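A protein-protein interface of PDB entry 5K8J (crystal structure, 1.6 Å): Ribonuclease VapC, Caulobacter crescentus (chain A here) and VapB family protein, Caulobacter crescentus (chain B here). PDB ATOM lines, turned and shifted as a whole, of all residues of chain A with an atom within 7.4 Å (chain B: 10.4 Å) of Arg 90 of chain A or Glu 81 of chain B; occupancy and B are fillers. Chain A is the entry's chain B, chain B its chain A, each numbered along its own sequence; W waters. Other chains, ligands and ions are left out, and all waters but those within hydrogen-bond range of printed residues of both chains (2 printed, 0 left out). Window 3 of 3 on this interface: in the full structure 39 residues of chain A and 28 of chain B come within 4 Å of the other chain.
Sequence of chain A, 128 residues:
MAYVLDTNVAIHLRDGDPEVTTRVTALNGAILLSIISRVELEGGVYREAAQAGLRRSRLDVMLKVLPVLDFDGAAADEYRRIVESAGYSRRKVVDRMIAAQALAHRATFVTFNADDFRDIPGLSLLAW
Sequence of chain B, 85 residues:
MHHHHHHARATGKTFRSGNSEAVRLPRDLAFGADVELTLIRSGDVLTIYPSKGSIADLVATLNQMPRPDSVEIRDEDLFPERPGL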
ATOM      1  N   TYR A  79      21.822   7.354  -0.234  1.00  0.00           N
ATOM      2  CA  TYR A  79      20.811   6.333  -0.026  1.00  0.00           C
ATOM      3  C   TYR A  79      19.860   6.279  -1.205  1.00  0.00           C
ATOM      4  O   TYR A  79      19.510   5.200  -1.679  1.00  0.00           O
ATOM      5  CB  TYR A  79      20.041   6.575   1.292  1.00  0.00           C
ATOM      6  CG  TYR A  79      19.011   5.514   1.584  1.00  0.00           C
ATOM      7  CD1 TYR A  79      19.340   4.386   2.339  1.00  0.00           C
ATOM      8  CD2 TYR A  79      17.717   5.602   1.075  1.00  0.00           C
ATOM      9  CE1 TYR A  79      18.423   3.386   2.569  1.00  0.00           C
ATOM     10  CE2 TYR A  79      16.790   4.597   1.310  1.00  0.00           C
ATOM     11  CZ  TYR A  79      17.158   3.489   2.067  1.00  0.00           C
ATOM     12  OH  TYR A  79      16.287   2.461   2.315  1.00  0.00           O
ATOM     13  N   GLY A  87      17.078  -1.355  -5.780  1.00  0.00           N
ATOM     14  CA  GLY A  87      15.707  -1.546  -5.384  1.00  0.00           C
ATOM     15  C   GLY A  87      15.558  -1.379  -3.891  1.00  0.00           C
ATOM     16  O   GLY A  87      16.511  -1.135  -3.156  1.00  0.00           O
ATOM     17  N   TYR A  88      14.326  -1.524  -3.433  1.00  0.00           N
ATOM     18  CA  TYR A  88      14.002  -1.308  -2.037  1.00  0.00           C
ATOM     19  C   TYR A  88      14.141  -2.591  -1.226  1.00  0.00           C
ATOM     20  O   TYR A  88      13.685  -3.662  -1.639  1.00  0.00           O
ATOM     21  CB  TYR A  88      12.575  -0.804  -1.908  1.00  0.00           C
ATOM     22  CG  TYR A  88      12.121  -0.633  -0.487  1.00  0.00           C
ATOM     23  CD1 TYR A  88      12.799   0.221   0.407  1.00  0.00           C
ATOM     24  CD2 TYR A  88      11.018  -1.326  -0.021  1.00  0.00           C
ATOM     25  CE1 TYR A  88      12.372   0.374   1.709  1.00  0.00           C
ATOM     26  CE2 TYR A  88      10.581  -1.172   1.299  1.00  0.00           C
ATOM     27  CZ  TYR A  88      11.251  -0.315   2.142  1.00  0.00           C
ATOM     28  OH  TYR A  88      10.814  -0.165   3.437  1.00  0.00           O
ATOM     29  N   SER A  89      14.745  -2.462  -0.049  1.00  0.00           N
ATOM     30  CA  SER A  89      14.820  -3.562   0.909  1.00  0.00           C
ATOM     31  C   SER A  89      14.510  -2.992   2.283  1.00  0.00           C
ATOM     32  O   SER A  89      15.332  -2.272   2.862  1.00  0.00           O
ATOM     33  CB  SER A  89      16.197  -4.218   0.912  1.00  0.00           C
ATOM     34  OG  SER A  89      16.341  -5.050   2.072  1.00  0.00           O
ATOM     35  N   ARG A  90      13.334  -3.307   2.819  1.00  0.00           N
ATOM     36  CA  ARG A  90      13.001  -2.818   4.156  1.00  0.00           C
ATOM     37  C   ARG A  90      13.995  -3.353   5.195  1.00  0.00           C
ATOM     38  O   ARG A  90      14.428  -2.614   6.099  1.00  0.00           O
ATOM     39  CB  ARG A  90      11.568  -3.237   4.528  1.00  0.00           C
ATOM     40  CG  ARG A  90      11.067  -2.547   5.823  1.00  0.00           C
ATOM     41  CD  ARG A  90       9.723  -3.176   6.326  1.00  0.00           C
ATOM     42  NE  ARG A  90       9.889  -4.614   6.484  1.00  0.00           N
ATOM     43  CZ  ARG A  90      10.644  -5.189   7.417  1.00  0.00           C
ATOM     44  NH1 ARG A  90      10.762  -6.507   7.448  1.00  0.00           N
ATOM     45  NH2 ARG A  90      11.274  -4.456   8.331  1.00  0.00           N
ATOM     46  N   ARG A  91      14.389  -4.619   5.048  1.00  0.00           N
ATOM     47  CA  ARG A  91      15.266  -5.296   6.013  1.00  0.00           C
ATOM     48  C   ARG A  91      16.635  -4.638   6.100  1.00  0.00           C
ATOM     49  O   ARG A  91      17.252  -4.632   7.169  1.00  0.00           O
ATOM     50  CB  ARG A  91      15.427  -6.768   5.645  1.00  0.00           C
ATOM     51  CG  ARG A  91      16.386  -7.518   6.535  1.00  0.00           C
ATOM     52  CD  ARG A  91      16.465  -9.001   6.130  1.00  0.00           C
ATOM     53  NE  ARG A  91      17.119  -9.175   4.835  1.00  0.00           N
ATOM     54  CZ  ARG A  91      18.438  -9.161   4.655  1.00  0.00           C
ATOM     55  NH1 ARG A  91      19.254  -8.973   5.688  1.00  0.00           N
ATOM     56  NH2 ARG A  91      18.939  -9.319   3.438  1.00  0.00           N
ATOM     57  N   LYS A  92      17.109  -4.032   5.012  1.00  0.00           N
ATOM     58  CA  LYS A  92      18.475  -3.510   4.960  1.00  0.00           C
ATOM     59  C   LYS A  92      18.549  -1.987   5.002  1.00  0.00           C
ATOM     60  O   LYS A  92      19.588  -1.411   4.667  1.00  0.00           O
ATOM     61  CB  LYS A  92      19.182  -4.060   3.718  1.00  0.00           C
ATOM     62  CG  LYS A  92      19.264  -5.586   3.680  1.00  0.00           C
ATOM     63  CD  LYS A  92      20.376  -6.068   2.747  1.00  0.00           C
ATOM     64  CE  LYS A  92      19.967  -5.916   1.311  1.00  0.00           C
ATOM     65  NZ  LYS A  92      21.046  -6.481   0.421  1.00  0.00           N
ATOM     66  N   VAL A  93      17.498  -1.298   5.453  1.00  0.00           N
ATOM     67  CA  VAL A  93      17.553   0.159   5.488  1.00  0.00           C
ATOM     68  C   VAL A  93      18.741   0.650   6.315  1.00  0.00           C
ATOM     69  O   VAL A  93      19.499   1.520   5.874  1.00  0.00           O
ATOM     70  CB  VAL A  93      16.223   0.762   5.991  1.00  0.00           C
ATOM     71  CG1 VAL A  93      16.363   2.252   6.199  1.00  0.00           C
ATOM     72  CG2 VAL A  93      15.093   0.449   5.018  1.00  0.00           C
ATOM     73  N   VAL A  94      18.893   0.160   7.551  1.00  0.00           N
ATOM     74  CA  VAL A  94      19.977   0.664   8.413  1.00  0.00           C
ATOM     75  C   VAL A  94      21.335   0.410   7.768  1.00  0.00           C
ATOM     76  O   VAL A  94      22.188   1.306   7.713  1.00  0.00           O
ATOM     77  CB  VAL A  94      19.915   0.019   9.809  1.00  0.00           C
ATOM     78  CG1 VAL A  94      21.190   0.357  10.581  1.00  0.00           C
ATOM     79  CG2 VAL A  94      18.707   0.532  10.565  1.00  0.00           C
ATOM     80  N   ARG A  96      22.065   0.144   4.649  1.00  0.00           N
ATOM     81  CA  ARG A  96      22.289   1.042   3.528  1.00  0.00           C
ATOM     82  C   ARG A  96      22.485   2.502   3.960  1.00  0.00           C
ATOM     83  O   ARG A  96      23.212   3.262   3.306  1.00  0.00           O
ATOM     84  CB  ARG A  96      21.118   0.870   2.555  1.00  0.00           C
ATOM     85  CG  ARG A  96      21.156  -0.450   1.823  1.00  0.00           C
ATOM     86  CD  ARG A  96      19.837  -0.724   1.149  1.00  0.00           C
ATOM     87  NE  ARG A  96      19.937  -1.896   0.290  1.00  0.00           N
ATOM     88  CZ  ARG A  96      19.014  -2.222  -0.610  1.00  0.00           C
ATOM     89  NH1 ARG A  96      17.953  -1.462  -0.734  1.00  0.00           N
ATOM     90  NH2 ARG A  96      19.158  -3.283  -1.405  1.00  0.00           N
ATOM     91  N   ASP B  75      19.918  -6.137  16.805  1.00  0.00           N
ATOM     92  CA  ASP B  75      18.745  -6.202  15.907  1.00  0.00           C
ATOM     93  C   ASP B  75      18.906  -5.183  14.763  1.00  0.00           C
ATOM     94  O   ASP B  75      18.713  -3.992  15.001  1.00  0.00           O
ATOM     95  CB  ASP B  75      17.450  -5.914  16.692  1.00  0.00           C
ATOM     96  CG  ASP B  75      17.580  -6.126  18.227  1.00  0.00           C
ATOM     97  OD1 ASP B  75      17.592  -7.293  18.699  1.00  0.00           O
ATOM     98  OD2 ASP B  75      17.593  -5.114  18.978  1.00  0.00           O
ATOM     99  N   GLU B  76      19.231  -5.618  13.508  1.00  0.00           N
ATOM    100  CA  GLU B  76      19.392  -4.637  12.396  1.00  0.00           C
ATOM    101  C   GLU B  76      18.069  -4.247  11.734  1.00  0.00           C
ATOM    102  O   GLU B  76      17.963  -3.152  11.120  1.00  0.00           O
ATOM    103  CB  GLU B  76      20.336  -5.156  11.284  1.00  0.00           C
ATOM    104  CG  GLU B  76      20.757  -4.117  10.197  1.00  0.00           C
ATOM    105  CD  GLU B  76      19.858  -4.086   8.919  1.00  0.00           C
ATOM    106  OE1 GLU B  76      19.968  -3.153   8.063  1.00  0.00           O
ATOM    107  OE2 GLU B  76      19.025  -5.005   8.783  1.00  0.00           O
ATOM    108  N   ASP B  77      17.062  -5.107  11.872  1.00  0.00           N
ATOM    109  CA  ASP B  77      15.791  -4.994  11.160  1.00  0.00           C
ATOM    110  C   ASP B  77      14.765  -4.224  12.000  1.00  0.00           C
ATOM    111  O   ASP B  77      13.823  -4.778  12.553  1.00  0.00           O
ATOM    112  CB  ASP B  77      15.284  -6.381  10.813  1.00  0.00           C
ATOM    113  CG  ASP B  77      14.075  -6.331   9.959  1.00  0.00           C
ATOM    114  OD1 ASP B  77      13.414  -7.379   9.827  1.00  0.00           O
ATOM    115  OD2 ASP B  77      13.779  -5.221   9.458  1.00  0.00           O
ATOM    116  N   LEU B  78      14.911  -2.898  11.959  1.00  0.00           N
ATOM    117  CA  LEU B  78      14.307  -1.876  12.799  1.00  0.00           C
ATOM    118  C   LEU B  78      13.225  -1.079  12.079  1.00  0.00           C
ATOM    119  O   LEU B  78      12.354  -0.490  12.744  1.00  0.00           O
ATOM    120  CB  LEU B  78      15.388  -0.920  13.294  1.00  0.00           C
ATOM    121  CG  LEU B  78      16.468  -1.544  14.176  1.00  0.00           C
ATOM    122  CD1 LEU B  78      17.451  -0.452  14.618  1.00  0.00           C
ATOM    123  CD2 LEU B  78      15.828  -2.224  15.366  1.00  0.00           C
ATOM    124  N   PHE B  79      13.255  -1.015  10.745  1.00  0.00           N
ATOM    125  CA  PHE B  79      12.337  -0.097  10.087  1.00  0.00           C
ATOM    126  C   PHE B  79      10.978  -0.748   9.922  1.00  0.00           C
ATOM    127  O   PHE B  79      10.887  -1.900   9.469  1.00  0.00           O
ATOM    128  CB  PHE B  79      12.892   0.390   8.748  1.00  0.00           C
ATOM    129  CG  PHE B  79      13.750   1.587   8.922  1.00  0.00           C
ATOM    130  CD1 PHE B  79      13.224   2.844   8.712  1.00  0.00           C
ATOM    131  CD2 PHE B  79      15.050   1.480   9.401  1.00  0.00           C
ATOM    132  CE1 PHE B  79      13.996   3.983   8.918  1.00  0.00           C
ATOM    133  CE2 PHE B  79      15.837   2.623   9.624  1.00  0.00           C
ATOM    134  CZ  PHE B  79      15.290   3.884   9.385  1.00  0.00           C
ATOM    135  N   PRO B  80       9.918  -0.079  10.345  1.00  0.00           N
ATOM    136  CA  PRO B  80       8.589  -0.668  10.255  1.00  0.00           C
ATOM    137  C   PRO B  80       8.053  -0.562   8.847  1.00  0.00           C
ATOM    138  O   PRO B  80       8.499   0.253   8.034  1.00  0.00           O
ATOM    139  CB  PRO B  80       7.755   0.171  11.231  1.00  0.00           C
ATOM    140  CG  PRO B  80       8.414   1.463  11.263  1.00  0.00           C
ATOM    141  CD  PRO B  80       9.887   1.250  10.981  1.00  0.00           C
ATOM    142  N   GLU B  81       7.083  -1.421   8.568  1.00  0.00           N
ATOM    143  CA  GLU B  81       6.363  -1.379   7.305  1.00  0.00           C
ATOM    144  C   GLU B  81       5.287  -0.314   7.427  1.00  0.00           C
ATOM    145  O   GLU B  81       4.314  -0.498   8.165  1.00  0.00           O
ATOM    146  CB  GLU B  81       5.752  -2.742   6.984  1.00  0.00           C
ATOM    147  CG  GLU B  81       5.169  -2.787   5.576  1.00  0.00           C
ATOM    148  CD  GLU B  81       4.601  -4.143   5.194  1.00  0.00           C
ATOM    149  OE1 GLU B  81       4.983  -5.153   5.823  1.00  0.00           O
ATOM    150  OE2 GLU B  81       3.767  -4.189   4.261  1.00  0.00           O
ATOM    151  N   ARG B  82       5.467   0.816   6.709  1.00  0.00           N
ATOM    152  CA  ARG B  82       4.521   1.928   6.726  1.00  0.00           C
ATOM    153  C   ARG B  82       3.488   1.762   5.617  1.00  0.00           C
ATOM    154  O   ARG B  82       3.863   1.618   4.444  1.00  0.00           O
ATOM    155  CB  ARG B  82       5.209   3.254   6.499  1.00  0.00           C
ATOM    156  CG  ARG B  82       6.433   3.503   7.316  1.00  0.00           C
ATOM    157  CD  ARG B  82       6.098   3.888   8.741  1.00  0.00           C
ATOM    158  NE  ARG B  82       7.281   4.468   9.344  1.00  0.00           N
ATOM    159  CZ  ARG B  82       7.399   4.831  10.613  1.00  0.00           C
ATOM    160  NH1 ARG B  82       6.410   4.637  11.486  1.00  0.00           N
ATOM    161  NH2 ARG B  82       8.525   5.375  11.015  1.00  0.00           N
ATOM    162  N   PRO B  83       2.208   1.865   5.921  1.00  0.00           N
ATOM    163  CA  PRO B  83       1.199   1.927   4.846  1.00  0.00           C
ATOM    164  C   PRO B  83       1.410   3.065   3.838  1.00  0.00           C
ATOM    165  O   PRO B  83       1.209   4.232   4.191  1.00  0.00           O
ATOM    166  CB  PRO B  83      -0.116   2.123   5.618  1.00  0.00           C
ATOM    167  CG  PRO B  83       0.152   1.744   7.015  1.00  0.00           C
ATOM    168  CD  PRO B  83       1.624   1.970   7.269  1.00  0.00           C
ATOM    169  N   GLY B  84       1.815   2.764   2.600  1.00  0.00           N
ATOM    170  CA  GLY B  84       1.546   3.649   1.473  1.00  0.00           C
ATOM    171  C   GLY B  84       2.681   4.441   0.802  1.00  0.00           C
ATOM    172  O   GLY B  84       2.375   5.326  -0.006  1.00  0.00           O
ATOM    173  N   LEU B  85       3.962   4.181   1.084  1.00  0.00           N
ATOM    174  CA  LEU B  85       5.028   4.796   0.240  1.00  0.00           C
ATOM    175  C   LEU B  85       5.579   3.766  -0.734  1.00  0.00           C
ATOM    176  O   LEU B  85       4.991   2.702  -0.912  1.00  0.00           O
ATOM    177  CB  LEU B  85       6.180   5.379   1.064  1.00  0.00           C
ATOM    178  CG  LEU B  85       6.688   4.520   2.261  1.00  0.00           C
ATOM    179  CD1 LEU B  85       7.202   3.108   1.939  1.00  0.00           C
ATOM    180  CD2 LEU B  85       7.752   5.256   3.046  1.00  0.00           C
HETATM  181  O   HOH W   1      16.904  -1.794   8.833  1.00  0.00           O
HETATM  182  O   HOH W   2      14.466  -2.765   8.685  1.00  0.00           O
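Tyr 88 of chain A touches none of the printed residues of chain B.
No residue of chain B comes within 4 Å of Ser 89 of chain A.
Of the printed residues of chain B, Arg 90 of chain A touches Asp 77, Phe 79, Pro 80 and Glu 81.
Printed residues of chain B within 4 Å of Arg 91 of chain A: Glu 76 and Asp 77.
Of the printed residues of chain B, Lys 92 of chain A touches Glu 76 (3.5 Å).
Printed residues of chain B within 4 Å of Val 94 of chain A: Glu 76 and Phe 79.
Glu 81 of chain B touches just one residue of chain A: Arg 90.
The nearest printed residue of chain B that does not touch Arg 90 of chain A is Leu 78 of chain B (5.4 Å).
The nearest printed residue of chain B that does not touch Val 93 of chain A is Glu 76 of chain B (4.04 Å).
Among the printed residues, pairs that only touch across the chains: Lys 92 of chain A with Glu 76 of chain B, Val 93 of chain A with Phe 79 of chain B, Val 94 of chain A with Glu 76 of chain B, Val 94 of chain A with Phe 79 of chain B, Arg 91 of chain A with Asp 77 of chain B, Arg 90 of chain A with Glu 81 of chain B and Arg 90 of chain A with Pro 80 of chain B.
Water W2 lies within hydrogen-bond range of the backbone carbonyl oxygen of Arg 90 of chain A (2.6 Å), the side-chain carboxylate of Asp 77 of chain B (2.7 Å), the backbone NH of Phe 79 of chain B (3.0 Å) and the backbone NH of Leu 78 of chain B (3.3 Å).
Water W1 lies within hydrogen-bond range of the backbone carbonyl oxygen of Glu 76 of chain B (2.9 Å), the backbone NH of Val 94 of chain A (3.1 Å), the backbone carbonyl oxygen of Arg 91 of chain A (3.3 Å) and the backbone NH of Val 93 of chain A (3.5 Å).
The backbone NH of Lys 92 of chain A lies within hydrogen-bond range of the side-chain hydroxyl of Ser 89 of chain A.
Of the 10 printed residues of chain A, 5 touch a printed residue of chain B.
Hydrophobic or aromatic side chains of chain B within 4 Å of the printed part of chain A: Phe 79.
Among the printed residues, Asp or Glu carboxylates within 4 Å of a Lys or Arg side-chain nitrogen of the other chain: Arg 90 of chain A with Asp 77 of chain B.
The side-chain carboxylate (OE2) of Glu 76 of chain B lies close to the backbone carbonyl oxygen (O) of Arg 91 of chain A (2.4 Å).
OD2 of Asp 77 of chain B is in salt-bridge range of NH2 of Arg 90 of chain A (2.9 Å).
O of Phe 79 of chain B lies within hydrogen-bond range of NH2 of Arg 90 of chain A.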
